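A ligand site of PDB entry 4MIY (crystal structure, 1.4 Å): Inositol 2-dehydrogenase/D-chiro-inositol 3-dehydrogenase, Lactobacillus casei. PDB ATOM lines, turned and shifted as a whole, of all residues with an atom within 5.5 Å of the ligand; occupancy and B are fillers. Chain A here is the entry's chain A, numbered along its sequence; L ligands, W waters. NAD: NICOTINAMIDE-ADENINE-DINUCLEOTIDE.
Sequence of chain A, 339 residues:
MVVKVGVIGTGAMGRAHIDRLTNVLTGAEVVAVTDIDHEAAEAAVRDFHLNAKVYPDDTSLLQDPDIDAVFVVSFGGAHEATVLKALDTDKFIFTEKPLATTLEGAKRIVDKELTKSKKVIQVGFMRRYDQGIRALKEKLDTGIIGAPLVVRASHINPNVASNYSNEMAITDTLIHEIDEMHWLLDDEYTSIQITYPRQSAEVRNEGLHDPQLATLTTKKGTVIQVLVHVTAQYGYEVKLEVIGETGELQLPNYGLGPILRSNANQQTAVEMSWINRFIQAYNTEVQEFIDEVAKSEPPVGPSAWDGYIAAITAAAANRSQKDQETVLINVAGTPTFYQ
The side-chain amino group (NZ) of Lys 97 is in hydrogen-bond range of an oxygen (O2D) of the ligand, at 3.3 Å.
O of Lys 97 is in hydrogen-bond range of O3D of the ligand (3.0 Å).
An oxygen (O2N) of the ligand is in hydrogen-bond range of the backbone NH (N) of Met 13.
An oxygen (O3D) of the ligand lies close to a ring nitrogen (NE2) of His 79.
An oxygen (O3B) of the ligand sits at hydrogen-bond distance from the side-chain carboxylate (OD2) of Asp 35 (2.6 Å).
N of Ala 12 is in hydrogen-bond range of O2A of the ligand, 3.1 Å away.
The backbone carbonyl oxygen (O) of Ser 74 sits close to an oxygen (O3D) of the ligand (3.4 Å).
The backbone NH (N) of Ile 36 sits at hydrogen-bond distance from a nitrogen (N3A) of the ligand, at 3.4 Å.
A nitrogen (N7N) of the ligand sits close to the side-chain sulfur (SD) of Met 126.
The side-chain hydroxyl (OH) of Tyr 282 lies within hydrogen-bond range of a nitrogen (N7N) of the ligand (2.7 Å).
N of Thr 10 is in hydrogen-bond range of OD2 of Asp 35 (2.8 Å).
NZ of Lys 97 is in salt-bridge range of OD1 of Asp 172 (3.5 Å).
O of Ile 8 is in hydrogen-bond range of N of Val 73 (2.8 Å).
The backbone NH (N) of Gly 9 sits at hydrogen-bond distance from the backbone carbonyl oxygen (O) of Thr 34.
The side-chain hydroxyl (OG1) of Thr 10 lies close to the backbone carbonyl oxygen (O) of Ala 40.
The backbone carbonyl oxygen (O) of Pro 98 is in hydrogen-bond range of a ring nitrogen (ND1) of His 79.
The backbone carbonyl oxygen (O) of Ser 74 lies within hydrogen-bond range of a ring nitrogen (NE2) of His 79 (2.9 Å).
A ring nitrogen (NE2) of His 79 lies close to the backbone carbonyl oxygen (O) of Phe 75.
OE1 of Glu 96 lies close to O7N of the ligand (2.9 Å).
The backbone carbonyl oxygen of Gly 124 sits close to an oxygen (O7N) of the ligand, at 3.4 Å.
Residues that only touch the ligand: Gly 11, Val 73, Phe 75, His 176, Gly 76, Ala 78, Gly 9, Thr 10, Ile 8 and Trp 274.
Hydrophobic or aromatic side chains within 4 Å of the ligand: Ile 8, Ala 12, Met 13, Ile 36, Val 73, Phe 75, Ala 78, His 79, Met 126, His 176, Trp 274 and Tyr 282.
Water W6 bridges a nitrogen (N1A) of the ligand (3.0 Å) and the backbone NH of Asp 58 (3.2 Å).
Water W10 lies within hydrogen-bond range of the backbone carbonyl oxygen of Val 73, the backbone NH of Gly 11, the backbone NH of Gly 14 and an oxygen (O2N) of the ligand.
Water W5 lies within hydrogen-bond range of O of Ala 78 (3.0 Å), N6A of the ligand (3.3 Å) and OG1 of Thr 82 (3.3 Å).
Water W4 bridges OG1 of Thr 34 and N of Asp 35.
Water W7 lies within hydrogen-bond range of OG1 of Thr 82 (2.6 Å), OG of Ser 74 (2.7 Å), O of Ala 78 (3.2 Å) and N6A of the ligand (3.5 Å).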
ATOM      1  N   ILE A   8      30.220   7.872 -10.391  1.00  0.00           N
ATOM      2  CA  ILE A   8      31.300   7.053  -9.946  1.00  0.00           C
ATOM      3  C   ILE A   8      30.776   6.104  -8.881  1.00  0.00           C
ATOM      4  O   ILE A   8      30.563   6.485  -7.748  1.00  0.00           O
ATOM      5  CB  ILE A   8      32.388   7.907  -9.355  1.00  0.00           C
ATOM      6  CG1 ILE A   8      32.843   8.940 -10.375  1.00  0.00           C
ATOM      7  CG2 ILE A   8      33.562   7.062  -8.872  1.00  0.00           C
ATOM      8  CD1 ILE A   8      33.604   9.987  -9.772  1.00  0.00           C
ATOM      9  N   GLY A   9      30.600   4.869  -9.292  1.00  0.00           N
ATOM     10  CA  GLY A   9      30.040   3.843  -8.458  1.00  0.00           C
ATOM     11  C   GLY A   9      28.663   3.571  -8.944  1.00  0.00           C
ATOM     12  O   GLY A   9      27.772   4.349  -8.700  1.00  0.00           O
ATOM     13  N   THR A  10      28.478   2.472  -9.625  1.00  0.00           N
ATOM     14  CA  THR A  10      27.193   2.127 -10.136  1.00  0.00           C
ATOM     15  C   THR A  10      26.610   0.870  -9.477  1.00  0.00           C
ATOM     16  O   THR A  10      26.267  -0.064 -10.124  1.00  0.00           O
ATOM     17  CB  THR A  10      27.223   1.985 -11.655  1.00  0.00           C
ATOM     18  OG1 THR A  10      28.114   0.943 -12.017  1.00  0.00           O
ATOM     19  CG2 THR A  10      27.749   3.226 -12.282  1.00  0.00           C
ATOM     20  N   GLY A  11      26.488   0.905  -8.181  1.00  0.00           N
ATOM     21  CA  GLY A  11      25.863  -0.180  -7.460  1.00  0.00           C
ATOM     22  C   GLY A  11      24.422   0.167  -7.215  1.00  0.00           C
ATOM     23  O   GLY A  11      23.787   0.770  -8.027  1.00  0.00           O
ATOM     24  N   ALA A  12      23.906  -0.273  -6.087  1.00  0.00           N
ATOM     25  CA  ALA A  12      22.514  -0.064  -5.746  1.00  0.00           C
ATOM     26  C   ALA A  12      22.082   1.416  -5.738  1.00  0.00           C
ATOM     27  O   ALA A  12      21.164   1.764  -6.395  1.00  0.00           O
ATOM     28  CB  ALA A  12      22.237  -0.685  -4.382  1.00  0.00           C
ATOM     29  N   MET A  13      22.759   2.221  -4.962  1.00  0.00           N
ATOM     30  CA  MET A  13      22.371   3.602  -4.800  1.00  0.00           C
ATOM     31  C   MET A  13      22.833   4.388  -6.011  1.00  0.00           C
ATOM     32  O   MET A  13      22.176   5.301  -6.443  1.00  0.00           O
ATOM     33  CB  MET A  13      22.945   4.136  -3.493  1.00  0.00           C
ATOM     34  CG  MET A  13      22.487   5.514  -3.106  1.00  0.00           C
ATOM     35  SD  MET A  13      20.689   5.572  -3.109  1.00  0.00           S
ATOM     36  CE  MET A  13      20.405   6.908  -1.993  1.00  0.00           C
ATOM     37  N   GLY A  14      23.942   3.973  -6.595  1.00  0.00           N
ATOM     38  CA  GLY A  14      24.372   4.571  -7.836  1.00  0.00           C
ATOM     39  C   GLY A  14      23.377   4.423  -8.944  1.00  0.00           C
ATOM     40  O   GLY A  14      23.097   5.337  -9.664  1.00  0.00           O
ATOM     41  N   THR A  34      31.683   5.209 -14.111  1.00  0.00           N
ATOM     42  CA  THR A  34      32.767   4.297 -13.825  1.00  0.00           C
ATOM     43  C   THR A  34      32.474   3.478 -12.581  1.00  0.00           C
ATOM     44  O   THR A  34      31.823   3.939 -11.672  1.00  0.00           O
ATOM     45  CB  THR A  34      34.107   5.033 -13.707  1.00  0.00           C
ATOM     46  OG1 THR A  34      35.174   4.089 -13.587  1.00  0.00           O
ATOM     47  CG2 THR A  34      34.167   5.944 -12.530  1.00  0.00           C
ATOM     48  N   ASP A  35      33.009   2.269 -12.529  1.00  0.00           N
ATOM     49  CA  ASP A  35      32.874   1.401 -11.388  1.00  0.00           C
ATOM     50  C   ASP A  35      34.142   0.533 -11.379  1.00  0.00           C
ATOM     51  O   ASP A  35      34.688   0.260 -12.417  1.00  0.00           O
ATOM     52  CB  ASP A  35      31.615   0.568 -11.591  1.00  0.00           C
ATOM     53  CG  ASP A  35      31.135  -0.147 -10.321  1.00  0.00           C
ATOM     54  OD1 ASP A  35      31.710  -1.154  -9.976  1.00  0.00           O
ATOM     55  OD2 ASP A  35      30.169   0.271  -9.700  1.00  0.00           O
ATOM     56  N   ILE A  36      34.647   0.121 -10.243  1.00  0.00           N
ATOM     57  CA  ILE A  36      35.756  -0.834 -10.269  1.00  0.00           C
ATOM     58  C   ILE A  36      35.342  -2.161 -10.752  1.00  0.00           C
ATOM     59  O   ILE A  36      36.191  -2.974 -11.042  1.00  0.00           O
ATOM     60  CB  ILE A  36      36.368  -1.032  -8.942  1.00  0.00           C
ATOM     61  CG1 ILE A  36      35.347  -1.643  -7.979  1.00  0.00           C
ATOM     62  CG2 ILE A  36      36.996   0.221  -8.476  1.00  0.00           C
ATOM     63  CD1 ILE A  36      35.817  -1.679  -6.592  1.00  0.00           C
ATOM     64  N   ASP A  37      34.039  -2.390 -10.822  1.00  0.00           N
ATOM     65  CA  ASP A  37      33.480  -3.528 -11.467  1.00  0.00           C
ATOM     66  C   ASP A  37      32.965  -3.098 -12.802  1.00  0.00           C
ATOM     67  O   ASP A  37      31.833  -2.750 -12.964  1.00  0.00           O
ATOM     68  CB  ASP A  37      32.384  -4.139 -10.615  1.00  0.00           C
ATOM     69  CG  ASP A  37      31.665  -5.323 -11.283  1.00  0.00           C
ATOM     70  OD1 ASP A  37      31.814  -5.573 -12.460  1.00  0.00           O
ATOM     71  OD2 ASP A  37      30.898  -5.991 -10.602  1.00  0.00           O
ATOM     72  N   ALA A  40      29.593  -3.816 -13.889  1.00  0.00           N
ATOM     73  CA  ALA A  40      28.524  -3.086 -13.286  1.00  0.00           C
ATOM     74  C   ALA A  40      28.302  -1.798 -14.063  1.00  0.00           C
ATOM     75  O   ALA A  40      27.177  -1.451 -14.360  1.00  0.00           O
ATOM     76  CB  ALA A  40      28.854  -2.808 -11.870  1.00  0.00           C
ATOM     77  N   ASP A  58      38.040   6.679 -11.915  1.00  0.00           N
ATOM     78  CA  ASP A  58      37.544   7.977 -11.542  1.00  0.00           C
ATOM     79  C   ASP A  58      38.428   9.068 -12.108  1.00  0.00           C
ATOM     80  O   ASP A  58      37.946  10.096 -12.520  1.00  0.00           O
ATOM     81  CB  ASP A  58      37.306   8.078 -10.033  1.00  0.00           C
ATOM     82  CG  ASP A  58      38.532   7.895  -9.241  1.00  0.00           C
ATOM     83  OD1 ASP A  58      39.531   7.441  -9.796  1.00  0.00           O
ATOM     84  OD2 ASP A  58      38.511   8.208  -8.041  1.00  0.00           O
ATOM     85  N   VAL A  73      29.197   7.634  -5.593  1.00  0.00           N
ATOM     86  CA  VAL A  73      28.318   6.655  -4.989  1.00  0.00           C
ATOM     87  C   VAL A  73      28.979   5.290  -4.818  1.00  0.00           C
ATOM     88  O   VAL A  73      28.360   4.297  -4.940  1.00  0.00           O
ATOM     89  CB  VAL A  73      27.009   6.513  -5.797  1.00  0.00           C
ATOM     90  CG1 VAL A  73      25.866   6.082  -4.887  1.00  0.00           C
ATOM     91  CG2 VAL A  73      26.626   7.814  -6.485  1.00  0.00           C
ATOM     92  N   SER A  74      30.269   5.318  -4.532  1.00  0.00           N
ATOM     93  CA  SER A  74      31.091   4.136  -4.368  1.00  0.00           C
ATOM     94  C   SER A  74      31.027   3.693  -2.905  1.00  0.00           C
ATOM     95  O   SER A  74      30.254   4.226  -2.160  1.00  0.00           O
ATOM     96  CB  SER A  74      32.504   4.463  -4.803  1.00  0.00           C
ATOM     97  OG  SER A  74      33.017   5.563  -4.155  1.00  0.00           O
ATOM     98  N   PHE A  75      31.837   2.728  -2.503  1.00  0.00           N
ATOM     99  CA  PHE A  75      31.909   2.372  -1.101  1.00  0.00           C
ATOM    100  C   PHE A  75      32.252   3.591  -0.299  1.00  0.00           C
ATOM    101  O   PHE A  75      32.957   4.440  -0.756  1.00  0.00           O
ATOM    102  CB  PHE A  75      32.981   1.305  -0.806  1.00  0.00           C
ATOM    103  CG  PHE A  75      32.820  -0.008  -1.535  1.00  0.00           C
ATOM    104  CD1 PHE A  75      31.612  -0.519  -1.890  1.00  0.00           C
ATOM    105  CD2 PHE A  75      33.957  -0.760  -1.841  1.00  0.00           C
ATOM    106  CE1 PHE A  75      31.510  -1.687  -2.528  1.00  0.00           C
ATOM    107  CE2 PHE A  75      33.865  -1.930  -2.470  1.00  0.00           C
ATOM    108  CZ  PHE A  75      32.643  -2.411  -2.824  1.00  0.00           C
ATOM    109  N   GLY A  76      31.762   3.685   0.919  1.00  0.00           N
ATOM    110  CA  GLY A  76      32.067   4.821   1.732  1.00  0.00           C
ATOM    111  C   GLY A  76      33.551   5.154   1.891  1.00  0.00           C
ATOM    112  O   GLY A  76      33.939   6.289   1.837  1.00  0.00           O
ATOM    113  N   ALA A  78      35.824   4.859   0.017  1.00  0.00           N
ATOM    114  CA  ALA A  78      36.398   5.285  -1.231  1.00  0.00           C
ATOM    115  C   ALA A  78      36.019   6.727  -1.602  1.00  0.00           C
ATOM    116  O   ALA A  78      36.429   7.203  -2.637  1.00  0.00           O
ATOM    117  CB  ALA A  78      35.966   4.388  -2.295  1.00  0.00           C
ATOM    118  N   HIS A  79      35.226   7.380  -0.776  1.00  0.00           N
ATOM    119  CA  HIS A  79      34.744   8.684  -1.147  1.00  0.00           C
ATOM    120  C   HIS A  79      35.812   9.722  -1.065  1.00  0.00           C
ATOM    121  O   HIS A  79      35.926  10.537  -1.941  1.00  0.00           O
ATOM    122  CB  HIS A  79      33.568   9.114  -0.285  1.00  0.00           C
ATOM    123  CG  HIS A  79      32.332   8.322  -0.510  1.00  0.00           C
ATOM    124  ND1 HIS A  79      31.167   8.560   0.190  1.00  0.00           N
ATOM    125  CD2 HIS A  79      32.049   7.313  -1.348  1.00  0.00           C
ATOM    126  CE1 HIS A  79      30.240   7.729  -0.222  1.00  0.00           C
ATOM    127  NE2 HIS A  79      30.751   6.948  -1.141  1.00  0.00           N
ATOM    128  N   THR A  82      38.350  10.137  -3.920  1.00  0.00           N
ATOM    129  CA  THR A  82      37.665  10.522  -5.121  1.00  0.00           C
ATOM    130  C   THR A  82      37.228  11.978  -5.053  1.00  0.00           C
ATOM    131  O   THR A  82      37.359  12.695  -6.013  1.00  0.00           O
ATOM    132  CB  THR A  82      36.509   9.602  -5.367  1.00  0.00           C
ATOM    133  OG1 THR A  82      36.999   8.300  -5.642  1.00  0.00           O
ATOM    134  CG2 THR A  82      35.660  10.083  -6.562  1.00  0.00           C
ATOM    135  N   GLU A  96      27.422  10.841  -1.938  1.00  0.00           N
ATOM    136  CA  GLU A  96      26.660  10.191  -0.908  1.00  0.00           C
ATOM    137  C   GLU A  96      27.389  10.257   0.425  1.00  0.00           C
ATOM    138  O   GLU A  96      28.578  10.450   0.483  1.00  0.00           O
ATOM    139  CB  GLU A  96      26.321   8.759  -1.289  1.00  0.00           C
ATOM    140  CG  GLU A  96      25.001   8.607  -2.028  1.00  0.00           C
ATOM    141  CD  GLU A  96      23.816   9.127  -1.228  1.00  0.00           C
ATOM    142  OE1 GLU A  96      23.923   9.240  -0.021  1.00  0.00           O
ATOM    143  OE2 GLU A  96      22.814   9.432  -1.822  1.00  0.00           O
ATOM    144  N   LYS A  97      26.645  10.087   1.502  1.00  0.00           N
ATOM    145  CA  LYS A  97      27.205   9.882   2.801  1.00  0.00           C
ATOM    146  C   LYS A  97      28.027   8.609   2.789  1.00  0.00           C
ATOM    147  O   LYS A  97      27.702   7.711   2.092  1.00  0.00           O
ATOM    148  CB  LYS A  97      26.104   9.732   3.836  1.00  0.00           C
ATOM    149  CG  LYS A  97      24.993   8.889   3.367  1.00  0.00           C
ATOM    150  CD  LYS A  97      24.595   7.805   4.295  1.00  0.00           C
ATOM    151  CE  LYS A  97      25.727   6.960   4.705  1.00  0.00           C
ATOM    152  NZ  LYS A  97      25.225   5.600   4.972  1.00  0.00           N
ATOM    153  N   PRO A  98      29.096   8.586   3.579  1.00  0.00           N
ATOM    154  CA  PRO A  98      29.680   9.688   4.322  1.00  0.00           C
ATOM    155  C   PRO A  98      30.581  10.558   3.432  1.00  0.00           C
ATOM    156  O   PRO A  98      30.941  10.122   2.367  1.00  0.00           O
ATOM    157  CB  PRO A  98      30.546   8.964   5.348  1.00  0.00           C
ATOM    158  CG  PRO A  98      30.965   7.841   4.638  1.00  0.00           C
ATOM    159  CD  PRO A  98      29.876   7.370   3.801  1.00  0.00           C
ATOM    160  N   GLY A 124      25.028  13.731   0.608  1.00  0.00           N
ATOM    161  CA  GLY A 124      23.714  13.140   0.517  1.00  0.00           C
ATOM    162  C   GLY A 124      22.895  12.870   1.782  1.00  0.00           C
ATOM    163  O   GLY A 124      22.305  11.826   1.877  1.00  0.00           O
ATOM    164  N   MET A 126      19.724  13.159   3.055  1.00  0.00           N
ATOM    165  CA  MET A 126      18.416  13.460   2.512  1.00  0.00           C
ATOM    166  C   MET A 126      17.323  13.817   3.508  1.00  0.00           C
ATOM    167  O   MET A 126      16.331  14.303   3.107  1.00  0.00           O
ATOM    168  CB  MET A 126      17.929  12.312   1.618  1.00  0.00           C
ATOM    169  CG  MET A 126      17.293  11.142   2.360  1.00  0.00           C
ATOM    170  SD  MET A 126      18.490  10.240   3.349  1.00  0.00           S
ATOM    171  CE  MET A 126      17.464   8.964   4.091  1.00  0.00           C
ATOM    172  N   ASP A 172      25.670   3.873   9.335  1.00  0.00           N
ATOM    173  CA  ASP A 172      24.648   3.695   8.323  1.00  0.00           C
ATOM    174  C   ASP A 172      23.254   4.155   8.780  1.00  0.00           C
ATOM    175  O   ASP A 172      22.453   4.547   7.998  1.00  0.00           O
ATOM    176  CB  ASP A 172      24.597   2.250   7.853  1.00  0.00           C
ATOM    177  CG  ASP A 172      25.749   1.890   6.930  1.00  0.00           C
ATOM    178  OD1 ASP A 172      26.523   2.776   6.566  1.00  0.00           O
ATOM    179  OD2 ASP A 172      25.877   0.732   6.565  1.00  0.00           O
ATOM    180  N   HIS A 176      22.024   9.547  10.109  1.00  0.00           N
ATOM    181  CA  HIS A 176      20.953  10.387   9.645  1.00  0.00           C
ATOM    182  C   HIS A 176      20.452  11.337  10.731  1.00  0.00           C
ATOM    183  O   HIS A 176      20.265  12.488  10.486  1.00  0.00           O
ATOM    184  CB  HIS A 176      19.823   9.530   9.072  1.00  0.00           C
ATOM    185  CG  HIS A 176      20.207   8.852   7.806  1.00  0.00           C
ATOM    186  ND1 HIS A 176      20.375   9.533   6.633  1.00  0.00           N
ATOM    187  CD2 HIS A 176      20.501   7.565   7.539  1.00  0.00           C
ATOM    188  CE1 HIS A 176      20.736   8.699   5.686  1.00  0.00           C
ATOM    189  NE2 HIS A 176      20.801   7.490   6.208  1.00  0.00           N
ATOM    190  N   TRP A 274      13.006   1.402   3.966  1.00  0.00           N
ATOM    191  CA  TRP A 274      13.501   2.768   4.039  1.00  0.00           C
ATOM    192  C   TRP A 274      13.603   3.381   2.663  1.00  0.00           C
ATOM    193  O   TRP A 274      13.542   4.556   2.517  1.00  0.00           O
ATOM    194  CB  TRP A 274      14.816   2.858   4.738  1.00  0.00           C
ATOM    195  CG  TRP A 274      15.877   1.953   4.225  1.00  0.00           C
ATOM    196  CD1 TRP A 274      16.178   0.749   4.704  1.00  0.00           C
ATOM    197  CD2 TRP A 274      16.782   2.218   3.171  1.00  0.00           C
ATOM    198  NE1 TRP A 274      17.204   0.207   3.995  1.00  0.00           N
ATOM    199  CE2 TRP A 274      17.599   1.101   3.047  1.00  0.00           C
ATOM    200  CE3 TRP A 274      16.963   3.267   2.302  1.00  0.00           C
ATOM    201  CZ2 TRP A 274      18.601   1.013   2.135  1.00  0.00           C
ATOM    202  CZ3 TRP A 274      17.936   3.169   1.379  1.00  0.00           C
ATOM    203  CH2 TRP A 274      18.762   2.055   1.301  1.00  0.00           C
ATOM    204  N   TYR A 282      14.890  11.864  -1.504  1.00  0.00           N
ATOM    205  CA  TYR A 282      15.926  11.677  -2.500  1.00  0.00           C
ATOM    206  C   TYR A 282      15.668  12.452  -3.761  1.00  0.00           C
ATOM    207  O   TYR A 282      16.536  13.066  -4.295  1.00  0.00           O
ATOM    208  CB  TYR A 282      16.155  10.194  -2.848  1.00  0.00           C
ATOM    209  CG  TYR A 282      16.648   9.308  -1.730  1.00  0.00           C
ATOM    210  CD1 TYR A 282      17.793   9.575  -1.058  1.00  0.00           C
ATOM    211  CD2 TYR A 282      15.993   8.155  -1.427  1.00  0.00           C
ATOM    212  CE1 TYR A 282      18.235   8.749  -0.059  1.00  0.00           C
ATOM    213  CE2 TYR A 282      16.409   7.340  -0.449  1.00  0.00           C
ATOM    214  CZ  TYR A 282      17.535   7.608   0.246  1.00  0.00           C
ATOM    215  OH  TYR A 282      17.927   6.746   1.233  1.00  0.00           O
HETATM  216  PA  NAD L   1      26.982  -0.984  -3.376  1.00  0.00           P
HETATM  217  O1A NAD L   1      28.011  -1.832  -2.804  1.00  0.00           O
HETATM  218  O2A NAD L   1      25.852  -1.511  -4.001  1.00  0.00           O
HETATM  219  O5B NAD L   1      27.554  -0.154  -4.603  1.00  0.00           O
HETATM  220  C5B NAD L   1      28.743   0.519  -4.603  1.00  0.00           C
HETATM  221  C4B NAD L   1      29.366   0.441  -5.996  1.00  0.00           C
HETATM  222  O4B NAD L   1      30.595   1.105  -5.912  1.00  0.00           O
HETATM  223  C3B NAD L   1      29.803  -0.954  -6.438  1.00  0.00           C
HETATM  224  O3B NAD L   1      29.358  -1.198  -7.704  1.00  0.00           O
HETATM  225  C2B NAD L   1      31.304  -0.955  -6.329  1.00  0.00           C
HETATM  226  O2B NAD L   1      31.917  -1.810  -7.265  1.00  0.00           O
HETATM  227  C1B NAD L   1      31.629   0.457  -6.662  1.00  0.00           C
HETATM  228  N9A NAD L   1      32.900   0.925  -6.166  1.00  0.00           N
HETATM  229  C8A NAD L   1      33.481   0.669  -5.040  1.00  0.00           C
HETATM  230  N7A NAD L   1      34.609   1.355  -4.871  1.00  0.00           N
HETATM  231  C5A NAD L   1      34.755   2.090  -5.960  1.00  0.00           C
HETATM  232  C6A NAD L   1      35.708   3.037  -6.491  1.00  0.00           C
HETATM  233  N6A NAD L   1      36.792   3.418  -5.847  1.00  0.00           N
HETATM  234  N1A NAD L   1      35.430   3.588  -7.644  1.00  0.00           N
HETATM  235  C2A NAD L   1      34.399   3.288  -8.338  1.00  0.00           C
HETATM  236  N3A NAD L   1      33.497   2.414  -7.949  1.00  0.00           N
HETATM  237  C4A NAD L   1      33.629   1.808  -6.783  1.00  0.00           C
HETATM  238  O3  NAD L   1      26.692   0.059  -2.227  1.00  0.00           O
HETATM  239  PN  NAD L   1      25.510   1.187  -2.203  1.00  0.00           P
HETATM  240  O1N NAD L   1      24.421   0.689  -1.363  1.00  0.00           O
HETATM  241  O2N NAD L   1      25.056   1.445  -3.522  1.00  0.00           O
HETATM  242  O5D NAD L   1      26.097   2.343  -1.409  1.00  0.00           O
HETATM  243  C5D NAD L   1      26.937   3.258  -2.067  1.00  0.00           C
HETATM  244  C4D NAD L   1      27.082   4.520  -1.272  1.00  0.00           C
HETATM  245  O4D NAD L   1      25.802   5.091  -1.151  1.00  0.00           O
HETATM  246  C3D NAD L   1      27.613   4.244   0.096  1.00  0.00           C
HETATM  247  O3D NAD L   1      28.424   5.318   0.471  1.00  0.00           O
HETATM  248  C2D NAD L   1      26.307   4.221   0.899  1.00  0.00           C
HETATM  249  O2D NAD L   1      26.617   4.578   2.194  1.00  0.00           O
HETATM  250  C1D NAD L   1      25.509   5.299   0.208  1.00  0.00           C
HETATM  251  N1N NAD L   1      24.071   5.168   0.461  1.00  0.00           N
HETATM  252  C2N NAD L   1      23.405   6.184   1.004  1.00  0.00           C
HETATM  253  C3N NAD L   1      22.066   6.126   1.307  1.00  0.00           C
HETATM  254  C7N NAD L   1      21.347   7.316   1.903  1.00  0.00           C
HETATM  255  O7N NAD L   1      21.743   8.425   1.766  1.00  0.00           O
HETATM  256  N7N NAD L   1      20.263   7.049   2.520  1.00  0.00           N
HETATM  257  C4N NAD L   1      21.392   4.962   0.994  1.00  0.00           C
HETATM  258  C5N NAD L   1      22.111   3.942   0.430  1.00  0.00           C
HETATM  259  C6N NAD L   1      23.449   4.068   0.187  1.00  0.00           C
HETATM  260  O   HOH W   1      28.597  -1.848  -0.353  1.00  0.00           O
HETATM  261  O   HOH W   2      28.394  -3.584  -8.124  1.00  0.00           O
HETATM  262  O   HOH W   3      25.079   0.642   1.710  1.00  0.00           O
HETATM  263  O   HOH W   4      36.085   3.232 -11.266  1.00  0.00           O
HETATM  264  O   HOH W   5      38.497   5.706  -4.231  1.00  0.00           O
HETATM  265  O   HOH W   6      37.506   4.721  -9.436  1.00  0.00           O
HETATM  266  O   HOH W   7      35.154   6.463  -5.532  1.00  0.00           O
HETATM  267  O   HOH W   8      21.039  10.895  -0.338  1.00  0.00           O
HETATM  268  O   HOH W   9      21.755   0.661  -0.993  1.00  0.00           O
HETATM  269  O   HOH W  10      26.389   2.586  -5.946  1.00  0.00           O
HETATM  270  O   HOH W  11      37.586   1.141  -3.500  1.00  0.00           O
